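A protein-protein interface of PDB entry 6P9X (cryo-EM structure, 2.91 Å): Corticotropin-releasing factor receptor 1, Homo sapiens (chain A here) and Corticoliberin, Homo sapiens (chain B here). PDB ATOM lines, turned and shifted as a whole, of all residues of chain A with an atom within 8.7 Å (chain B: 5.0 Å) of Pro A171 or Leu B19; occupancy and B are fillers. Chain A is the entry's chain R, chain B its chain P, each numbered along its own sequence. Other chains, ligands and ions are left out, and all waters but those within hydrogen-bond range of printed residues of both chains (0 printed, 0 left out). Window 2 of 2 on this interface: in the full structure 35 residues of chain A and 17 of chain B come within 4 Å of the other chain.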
ATOM      1  N   HIS A 110     -20.139  31.098 -28.813  1.00  0.00           N
ATOM      2  CA  HIS A 110     -19.689  31.200 -30.197  1.00  0.00           C
ATOM      3  C   HIS A 110     -19.196  32.603 -30.523  1.00  0.00           C
ATOM      4  O   HIS A 110     -18.461  32.788 -31.497  1.00  0.00           O
ATOM      5  CB  HIS A 110     -20.818  30.801 -31.145  1.00  0.00           C
ATOM      6  CG  HIS A 110     -21.135  29.339 -31.123  1.00  0.00           C
ATOM      7  ND1 HIS A 110     -22.419  28.856 -31.245  1.00  0.00           N
ATOM      8  CD2 HIS A 110     -20.335  28.256 -30.996  1.00  0.00           C
ATOM      9  CE1 HIS A 110     -22.397  27.536 -31.192  1.00  0.00           C
ATOM     10  NE2 HIS A 110     -21.145  27.146 -31.043  1.00  0.00           N
ATOM     11  N   VAL A 165      -4.087  23.969 -31.666  1.00  0.00           N
ATOM     12  CA  VAL A 165      -5.077  23.345 -30.795  1.00  0.00           C
ATOM     13  C   VAL A 165      -6.488  23.644 -31.289  1.00  0.00           C
ATOM     14  O   VAL A 165      -7.419  22.868 -31.058  1.00  0.00           O
ATOM     15  CB  VAL A 165      -4.871  23.802 -29.338  1.00  0.00           C
ATOM     16  CG1 VAL A 165      -5.832  23.091 -28.406  1.00  0.00           C
ATOM     17  CG2 VAL A 165      -3.444  23.536 -28.901  1.00  0.00           C
ATOM     18  N   GLN A 166      -6.669  24.762 -31.991  1.00  0.00           N
ATOM     19  CA  GLN A 166      -8.010  25.124 -32.438  1.00  0.00           C
ATOM     20  C   GLN A 166      -8.411  24.354 -33.689  1.00  0.00           C
ATOM     21  O   GLN A 166      -9.580  23.982 -33.845  1.00  0.00           O
ATOM     22  CB  GLN A 166      -8.095  26.627 -32.680  1.00  0.00           C
ATOM     23  CG  GLN A 166      -8.264  27.432 -31.411  1.00  0.00           C
ATOM     24  CD  GLN A 166      -9.598  27.192 -30.741  1.00  0.00           C
ATOM     25  OE1 GLN A 166      -9.705  27.228 -29.518  1.00  0.00           O
ATOM     26  NE2 GLN A 166     -10.628  26.950 -31.542  1.00  0.00           N
ATOM     27  N   THR A 168      -6.837  21.378 -34.984  1.00  0.00           N
ATOM     28  CA  THR A 168      -6.659  19.935 -34.900  1.00  0.00           C
ATOM     29  C   THR A 168      -7.434  19.300 -33.750  1.00  0.00           C
ATOM     30  O   THR A 168      -7.078  18.200 -33.312  1.00  0.00           O
ATOM     31  CB  THR A 168      -5.174  19.591 -34.779  1.00  0.00           C
ATOM     32  OG1 THR A 168      -4.722  19.882 -33.453  1.00  0.00           O
ATOM     33  CG2 THR A 168      -4.360  20.397 -35.777  1.00  0.00           C
ATOM     34  N   MET A 169      -8.475  19.958 -33.250  1.00  0.00           N
ATOM     35  CA  MET A 169      -9.358  19.376 -32.250  1.00  0.00           C
ATOM     36  C   MET A 169     -10.756  19.212 -32.828  1.00  0.00           C
ATOM     37  O   MET A 169     -11.203  20.010 -33.657  1.00  0.00           O
ATOM     38  CB  MET A 169      -9.427  20.232 -30.984  1.00  0.00           C
ATOM     39  CG  MET A 169      -8.207  20.138 -30.088  1.00  0.00           C
ATOM     40  SD  MET A 169      -7.897  18.523 -29.366  1.00  0.00           S
ATOM     41  CE  MET A 169      -6.353  18.861 -28.520  1.00  0.00           C
ATOM     42  N   SER A 170     -11.442  18.171 -32.373  1.00  0.00           N
ATOM     43  CA  SER A 170     -12.779  17.842 -32.841  1.00  0.00           C
ATOM     44  C   SER A 170     -13.363  16.798 -31.902  1.00  0.00           C
ATOM     45  O   SER A 170     -12.615  16.116 -31.192  1.00  0.00           O
ATOM     46  CB  SER A 170     -12.748  17.317 -34.286  1.00  0.00           C
ATOM     47  OG  SER A 170     -12.062  16.082 -34.362  1.00  0.00           O
ATOM     48  N   PRO A 171     -14.690  16.656 -31.864  1.00  0.00           N
ATOM     49  CA  PRO A 171     -15.283  15.614 -31.010  1.00  0.00           C
ATOM     50  C   PRO A 171     -14.848  14.208 -31.381  1.00  0.00           C
ATOM     51  O   PRO A 171     -15.049  13.283 -30.586  1.00  0.00           O
ATOM     52  CB  PRO A 171     -16.792  15.808 -31.209  1.00  0.00           C
ATOM     53  CG  PRO A 171     -16.925  16.612 -32.460  1.00  0.00           C
ATOM     54  CD  PRO A 171     -15.718  17.486 -32.512  1.00  0.00           C
ATOM     55  N   GLU A 172     -14.257  14.017 -32.562  1.00  0.00           N
ATOM     56  CA  GLU A 172     -13.711  12.712 -32.919  1.00  0.00           C
ATOM     57  C   GLU A 172     -12.371  12.475 -32.234  1.00  0.00           C
ATOM     58  O   GLU A 172     -12.138  11.408 -31.654  1.00  0.00           O
ATOM     59  CB  GLU A 172     -13.565  12.604 -34.436  1.00  0.00           C
ATOM     60  CG  GLU A 172     -14.793  12.065 -35.149  1.00  0.00           C
ATOM     61  CD  GLU A 172     -14.553  11.844 -36.630  1.00  0.00           C
ATOM     62  OE1 GLU A 172     -13.607  12.450 -37.176  1.00  0.00           O
ATOM     63  OE2 GLU A 172     -15.307  11.063 -37.248  1.00  0.00           O
ATOM     64  N   VAL A 173     -11.476  13.463 -32.291  1.00  0.00           N
ATOM     65  CA  VAL A 173     -10.158  13.309 -31.683  1.00  0.00           C
ATOM     66  C   VAL A 173     -10.254  13.394 -30.165  1.00  0.00           C
ATOM     67  O   VAL A 173      -9.449  12.792 -29.445  1.00  0.00           O
ATOM     68  CB  VAL A 173      -9.186  14.360 -32.249  1.00  0.00           C
ATOM     69  CG1 VAL A 173      -7.759  14.023 -31.869  1.00  0.00           C
ATOM     70  CG2 VAL A 173      -9.329  14.452 -33.756  1.00  0.00           C
ATOM     71  N   HIS A 174     -11.234  14.142 -29.655  1.00  0.00           N
ATOM     72  CA  HIS A 174     -11.409  14.265 -28.212  1.00  0.00           C
ATOM     73  C   HIS A 174     -11.715  12.913 -27.579  1.00  0.00           C
ATOM     74  O   HIS A 174     -11.115  12.536 -26.567  1.00  0.00           O
ATOM     75  CB  HIS A 174     -12.522  15.270 -27.910  1.00  0.00           C
ATOM     76  CG  HIS A 174     -12.569  15.715 -26.482  1.00  0.00           C
ATOM     77  ND1 HIS A 174     -11.471  16.222 -25.823  1.00  0.00           N
ATOM     78  CD2 HIS A 174     -13.588  15.743 -25.592  1.00  0.00           C
ATOM     79  CE1 HIS A 174     -11.809  16.537 -24.586  1.00  0.00           C
ATOM     80  NE2 HIS A 174     -13.087  16.255 -24.419  1.00  0.00           N
ATOM     81  N   GLN A 175     -12.648  12.164 -28.169  1.00  0.00           N
ATOM     82  CA  GLN A 175     -12.971  10.836 -27.660  1.00  0.00           C
ATOM     83  C   GLN A 175     -11.905   9.812 -28.025  1.00  0.00           C
ATOM     84  O   GLN A 175     -11.731   8.821 -27.307  1.00  0.00           O
ATOM     85  CB  GLN A 175     -14.332  10.390 -28.198  1.00  0.00           C
ATOM     86  CG  GLN A 175     -14.849   9.093 -27.602  1.00  0.00           C
ATOM     87  CD  GLN A 175     -16.016   8.521 -28.380  1.00  0.00           C
ATOM     88  OE1 GLN A 175     -16.714   7.626 -27.905  1.00  0.00           O
ATOM     89  NE2 GLN A 175     -16.230   9.034 -29.586  1.00  0.00           N
ATOM     90  N   SER A 176     -11.181  10.036 -29.124  1.00  0.00           N
ATOM     91  CA  SER A 176     -10.164   9.086 -29.560  1.00  0.00           C
ATOM     92  C   SER A 176      -9.011   8.986 -28.571  1.00  0.00           C
ATOM     93  O   SER A 176      -8.492   7.886 -28.345  1.00  0.00           O
ATOM     94  CB  SER A 176      -9.636   9.483 -30.939  1.00  0.00           C
ATOM     95  OG  SER A 176      -8.419   8.819 -31.229  1.00  0.00           O
ATOM     96  N   ASN A 177      -8.597  10.110 -27.982  1.00  0.00           N
ATOM     97  CA  ASN A 177      -7.448  10.165 -27.078  1.00  0.00           C
ATOM     98  C   ASN A 177      -6.188   9.646 -27.776  1.00  0.00           C
ATOM     99  O   ASN A 177      -5.457   8.796 -27.264  1.00  0.00           O
ATOM    100  CB  ASN A 177      -7.730   9.396 -25.782  1.00  0.00           C
ATOM    101  CG  ASN A 177      -6.689   9.651 -24.715  1.00  0.00           C
ATOM    102  OD1 ASN A 177      -5.918  10.601 -24.802  1.00  0.00           O
ATOM    103  ND2 ASN A 177      -6.663   8.799 -23.697  1.00  0.00           N
ATOM    104  N   CYS A 181      -2.636  13.919 -29.894  1.00  0.00           N
ATOM    105  CA  CYS A 181      -3.541  14.850 -29.231  1.00  0.00           C
ATOM    106  C   CYS A 181      -3.010  15.247 -27.860  1.00  0.00           C
ATOM    107  O   CYS A 181      -3.029  16.429 -27.501  1.00  0.00           O
ATOM    108  CB  CYS A 181      -4.930  14.227 -29.102  1.00  0.00           C
ATOM    109  SG  CYS A 181      -6.272  15.402 -28.875  1.00  0.00           S
ATOM    110  N   LYS A 250      -9.486  11.985 -22.658  1.00  0.00           N
ATOM    111  CA  LYS A 250     -10.012  13.187 -23.304  1.00  0.00           C
ATOM    112  C   LYS A 250      -8.899  14.166 -23.676  1.00  0.00           C
ATOM    113  O   LYS A 250      -8.967  15.359 -23.379  1.00  0.00           O
ATOM    114  CB  LYS A 250     -11.059  13.869 -22.421  1.00  0.00           C
ATOM    115  CG  LYS A 250     -12.317  13.053 -22.204  1.00  0.00           C
ATOM    116  CD  LYS A 250     -13.479  13.942 -21.801  1.00  0.00           C
ATOM    117  CE  LYS A 250     -14.569  13.141 -21.120  1.00  0.00           C
ATOM    118  NZ  LYS A 250     -14.107  12.603 -19.810  1.00  0.00           N
ATOM    119  N   CYS A 251      -7.867  13.648 -24.335  1.00  0.00           N
ATOM    120  CA  CYS A 251      -6.750  14.430 -24.857  1.00  0.00           C
ATOM    121  C   CYS A 251      -6.043  15.250 -23.784  1.00  0.00           C
ATOM    122  O   CYS A 251      -5.407  16.261 -24.105  1.00  0.00           O
ATOM    123  CB  CYS A 251      -7.199  15.348 -25.999  1.00  0.00           C
ATOM    124  SG  CYS A 251      -7.510  14.491 -27.550  1.00  0.00           S
ATOM    125  N   PHE A 253      -6.956  17.375 -21.681  1.00  0.00           N
ATOM    126  CA  PHE A 253      -7.551  18.638 -21.266  1.00  0.00           C
ATOM    127  C   PHE A 253      -9.008  18.503 -20.853  1.00  0.00           C
ATOM    128  O   PHE A 253      -9.670  19.520 -20.627  1.00  0.00           O
ATOM    129  CB  PHE A 253      -7.401  19.700 -22.368  1.00  0.00           C
ATOM    130  CG  PHE A 253      -8.264  19.473 -23.577  1.00  0.00           C
ATOM    131  CD1 PHE A 253      -9.537  20.013 -23.650  1.00  0.00           C
ATOM    132  CD2 PHE A 253      -7.788  18.758 -24.658  1.00  0.00           C
ATOM    133  CE1 PHE A 253     -10.326  19.815 -24.762  1.00  0.00           C
ATOM    134  CE2 PHE A 253      -8.573  18.561 -25.773  1.00  0.00           C
ATOM    135  CZ  PHE A 253      -9.842  19.091 -25.826  1.00  0.00           C
ATOM    136  N   GLY A 254      -9.523  17.283 -20.738  1.00  0.00           N
ATOM    137  CA  GLY A 254     -10.843  17.078 -20.180  1.00  0.00           C
ATOM    138  C   GLY A 254     -10.803  17.089 -18.667  1.00  0.00           C
ATOM    139  O   GLY A 254     -10.036  16.336 -18.060  1.00  0.00           O
ATOM    140  N   LEU B  15     -12.858  25.309 -25.250  1.00  0.00           N
ATOM    141  CA  LEU B  15     -12.770  24.100 -26.058  1.00  0.00           C
ATOM    142  C   LEU B  15     -13.659  23.001 -25.495  1.00  0.00           C
ATOM    143  O   LEU B  15     -14.329  22.288 -26.250  1.00  0.00           O
ATOM    144  CB  LEU B  15     -11.319  23.629 -26.141  1.00  0.00           C
ATOM    145  CG  LEU B  15     -10.895  22.944 -27.438  1.00  0.00           C
ATOM    146  CD1 LEU B  15     -10.970  23.916 -28.600  1.00  0.00           C
ATOM    147  CD2 LEU B  15      -9.497  22.374 -27.309  1.00  0.00           C
ATOM    148  N   ARG B  16     -13.687  22.852 -24.171  1.00  0.00           N
ATOM    149  CA  ARG B  16     -14.529  21.827 -23.564  1.00  0.00           C
ATOM    150  C   ARG B  16     -16.006  22.161 -23.723  1.00  0.00           C
ATOM    151  O   ARG B  16     -16.857  21.263 -23.723  1.00  0.00           O
ATOM    152  CB  ARG B  16     -14.177  21.663 -22.086  1.00  0.00           C
ATOM    153  CG  ARG B  16     -13.026  20.716 -21.819  1.00  0.00           C
ATOM    154  CD  ARG B  16     -12.936  20.375 -20.343  1.00  0.00           C
ATOM    155  NE  ARG B  16     -12.858  21.568 -19.506  1.00  0.00           N
ATOM    156  CZ  ARG B  16     -11.723  22.114 -19.085  1.00  0.00           C
ATOM    157  NH1 ARG B  16     -10.559  21.576 -19.421  1.00  0.00           N
ATOM    158  NH2 ARG B  16     -11.749  23.199 -18.327  1.00  0.00           N
ATOM    159  N   GLU B  17     -16.332  23.447 -23.855  1.00  0.00           N
ATOM    160  CA  GLU B  17     -17.730  23.842 -23.995  1.00  0.00           C
ATOM    161  C   GLU B  17     -18.249  23.548 -25.395  1.00  0.00           C
ATOM    162  O   GLU B  17     -19.391  23.105 -25.558  1.00  0.00           O
ATOM    163  CB  GLU B  17     -17.896  25.324 -23.664  1.00  0.00           C
ATOM    164  CG  GLU B  17     -17.874  25.640 -22.177  1.00  0.00           C
ATOM    165  CD  GLU B  17     -18.448  24.524 -21.330  1.00  0.00           C
ATOM    166  OE1 GLU B  17     -19.687  24.382 -21.290  1.00  0.00           O
ATOM    167  OE2 GLU B  17     -17.658  23.790 -20.699  1.00  0.00           O
ATOM    168  N   VAL B  18     -17.430  23.790 -26.419  1.00  0.00           N
ATOM    169  CA  VAL B  18     -17.871  23.560 -27.792  1.00  0.00           C
ATOM    170  C   VAL B  18     -17.801  22.075 -28.134  1.00  0.00           C
ATOM    171  O   VAL B  18     -18.554  21.579 -28.977  1.00  0.00           O
ATOM    172  CB  VAL B  18     -17.047  24.405 -28.778  1.00  0.00           C
ATOM    173  CG1 VAL B  18     -17.236  25.884 -28.496  1.00  0.00           C
ATOM    174  CG2 VAL B  18     -15.579  24.033 -28.710  1.00  0.00           C
ATOM    175  N   LEU B  19     -16.903  21.341 -27.477  1.00  0.00           N
ATOM    176  CA  LEU B  19     -16.742  19.923 -27.772  1.00  0.00           C
ATOM    177  C   LEU B  19     -17.894  19.112 -27.192  1.00  0.00           C
ATOM    178  O   LEU B  19     -18.104  17.958 -27.579  1.00  0.00           O
ATOM    179  CB  LEU B  19     -15.403  19.407 -27.244  1.00  0.00           C
ATOM    180  CG  LEU B  19     -14.190  19.732 -28.115  1.00  0.00           C
ATOM    181  CD1 LEU B  19     -12.978  18.939 -27.668  1.00  0.00           C
ATOM    182  CD2 LEU B  19     -14.494  19.472 -29.577  1.00  0.00           C
ATOM    183  N   GLU B  20     -18.641  19.699 -26.257  1.00  0.00           N
ATOM    184  CA  GLU B  20     -19.891  19.118 -25.801  1.00  0.00           C
ATOM    185  C   GLU B  20     -21.109  19.846 -26.344  1.00  0.00           C
ATOM    186  O   GLU B  20     -22.233  19.373 -26.144  1.00  0.00           O
ATOM    187  CB  GLU B  20     -19.963  19.095 -24.265  1.00  0.00           C
ATOM    188  CG  GLU B  20     -20.077  20.461 -23.617  1.00  0.00           C
ATOM    189  CD  GLU B  20     -20.117  20.380 -22.103  1.00  0.00           C
ATOM    190  OE1 GLU B  20     -20.028  19.255 -21.567  1.00  0.00           O
ATOM    191  OE2 GLU B  20     -20.239  21.437 -21.449  1.00  0.00           O
ATOM    192  N   MET B  21     -20.919  20.980 -27.016  1.00  0.00           N
ATOM    193  CA  MET B  21     -21.991  21.683 -27.704  1.00  0.00           C
ATOM    194  C   MET B  21     -22.076  21.322 -29.180  1.00  0.00           C
ATOM    195  O   MET B  21     -23.184  21.122 -29.689  1.00  0.00           O
ATOM    196  CB  MET B  21     -21.807  23.197 -27.551  1.00  0.00           C
ATOM    197  CG  MET B  21     -22.709  24.043 -28.421  1.00  0.00           C
ATOM    198  SD  MET B  21     -22.654  25.773 -27.922  1.00  0.00           S
ATOM    199  CE  MET B  21     -20.889  26.063 -27.914  1.00  0.00           C
ATOM    200  N   ALA B  22     -20.942  21.220 -29.873  1.00  0.00           N
ATOM    201  CA  ALA B  22     -20.924  20.736 -31.247  1.00  0.00           C
ATOM    202  C   ALA B  22     -21.206  19.248 -31.349  1.00  0.00           C
ATOM    203  O   ALA B  22     -21.598  18.775 -32.419  1.00  0.00           O
ATOM    204  CB  ALA B  22     -19.574  21.035 -31.907  1.00  0.00           C
ATOM    205  N   ARG B  23     -21.012  18.502 -30.261  1.00  0.00           N
ATOM    206  CA  ARG B  23     -21.354  17.085 -30.252  1.00  0.00           C
ATOM    207  C   ARG B  23     -22.857  16.877 -30.115  1.00  0.00           C
ATOM    208  O   ARG B  23     -23.408  15.924 -30.676  1.00  0.00           O
ATOM    209  CB  ARG B  23     -20.609  16.378 -29.121  1.00  0.00           C
ATOM    210  CG  ARG B  23     -20.800  14.874 -29.091  1.00  0.00           C
ATOM    211  CD  ARG B  23     -20.156  14.271 -27.856  1.00  0.00           C
ATOM    212  NE  ARG B  23     -20.842  14.673 -26.632  1.00  0.00           N
ATOM    213  CZ  ARG B  23     -20.319  14.572 -25.416  1.00  0.00           C
ATOM    214  NH1 ARG B  23     -19.097  14.084 -25.255  1.00  0.00           N
ATOM    215  NH2 ARG B  23     -21.016  14.962 -24.358  1.00  0.00           N
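Printed residues of chain B that touch a printed residue of chain A: Leu B15, Arg B16, Leu B19 and Met B21. Hydrophobic or aromatic side chains of chain B that line the printed part of chain A: Leu B15, Leu B19 and Met B21. Of the 18 printed residues of chain A, 9 touch a printed residue of chain B. Hydrophobic or aromatic side chains of chain A that line the printed part of chain B: His A110, Val A165, Met A169, Pro A171, His A174 and Phe A253. Along chain A the printed residues that touch a printed residue of chain B span positions 110 to 254.
OG of Ser A170 sits close to N of Val A173, 3.4 Å away. The side-chain sulfur of Cys A181 is disulfide-bonded to the side-chain sulfur of Cys A251, at 2.0 Å.
A ring nitrogen (NE2) of His A110 lies close to the side-chain sulfur (SD) of Met B21 (3.7 Å). The guanidinium group of Arg B16 lies within hydrogen-bond range of the backbone carbonyl oxygen of Phe A253, at 2.5 Å.
Of the printed residues of chain B, Pro A171 touches Leu B19 (3.6 Å). Leu B19 touches four residues of chain A. Of the printed residues of chain B, Gln A166 touches Leu B15 (3.7 Å). Of the printed residues of chain B, His A110 touches Met B21 (3.3 Å). Of the printed residues of chain B, Ser A170 touches Leu B19. Of the printed residues of chain B, Gly A254 touches Arg B16 (3.9 Å). Of the printed residues of chain A, Arg B16 touches Phe A253 (2.5 Å) and Gly A254 (3.9 Å). Val A173 touches none of the printed residues of chain B. Lys A250 touches none of the printed residues of chain B. The nearest residue of chain B that does not touch Pro A171 is Arg B23 (4.4 Å). The nearest residue of chain A that does not touch Leu B19 is Met A169 (5.0 Å). The nearest printed residue of chain B that does not touch His A174 is Arg B16 (5.2 Å).
Leu B15 touches Val A165. OE1 of Gln A166 touches CD1 of Leu B15, 3.7 Å away. Leu B15 touches Met A169 (CD2 to CG, 3.8 Å). Ser A170 touches Leu B19 (C to CD2, 3.7 Å). Leu B19 touches Pro A171. His A174 touches Leu B19. Phe A253 touches Leu B15 (CZ to CD2, 3.6 Å). Leu B19 touches Phe A253. CA of Gly A254 touches CD of Arg B16, 3.9 Å away.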
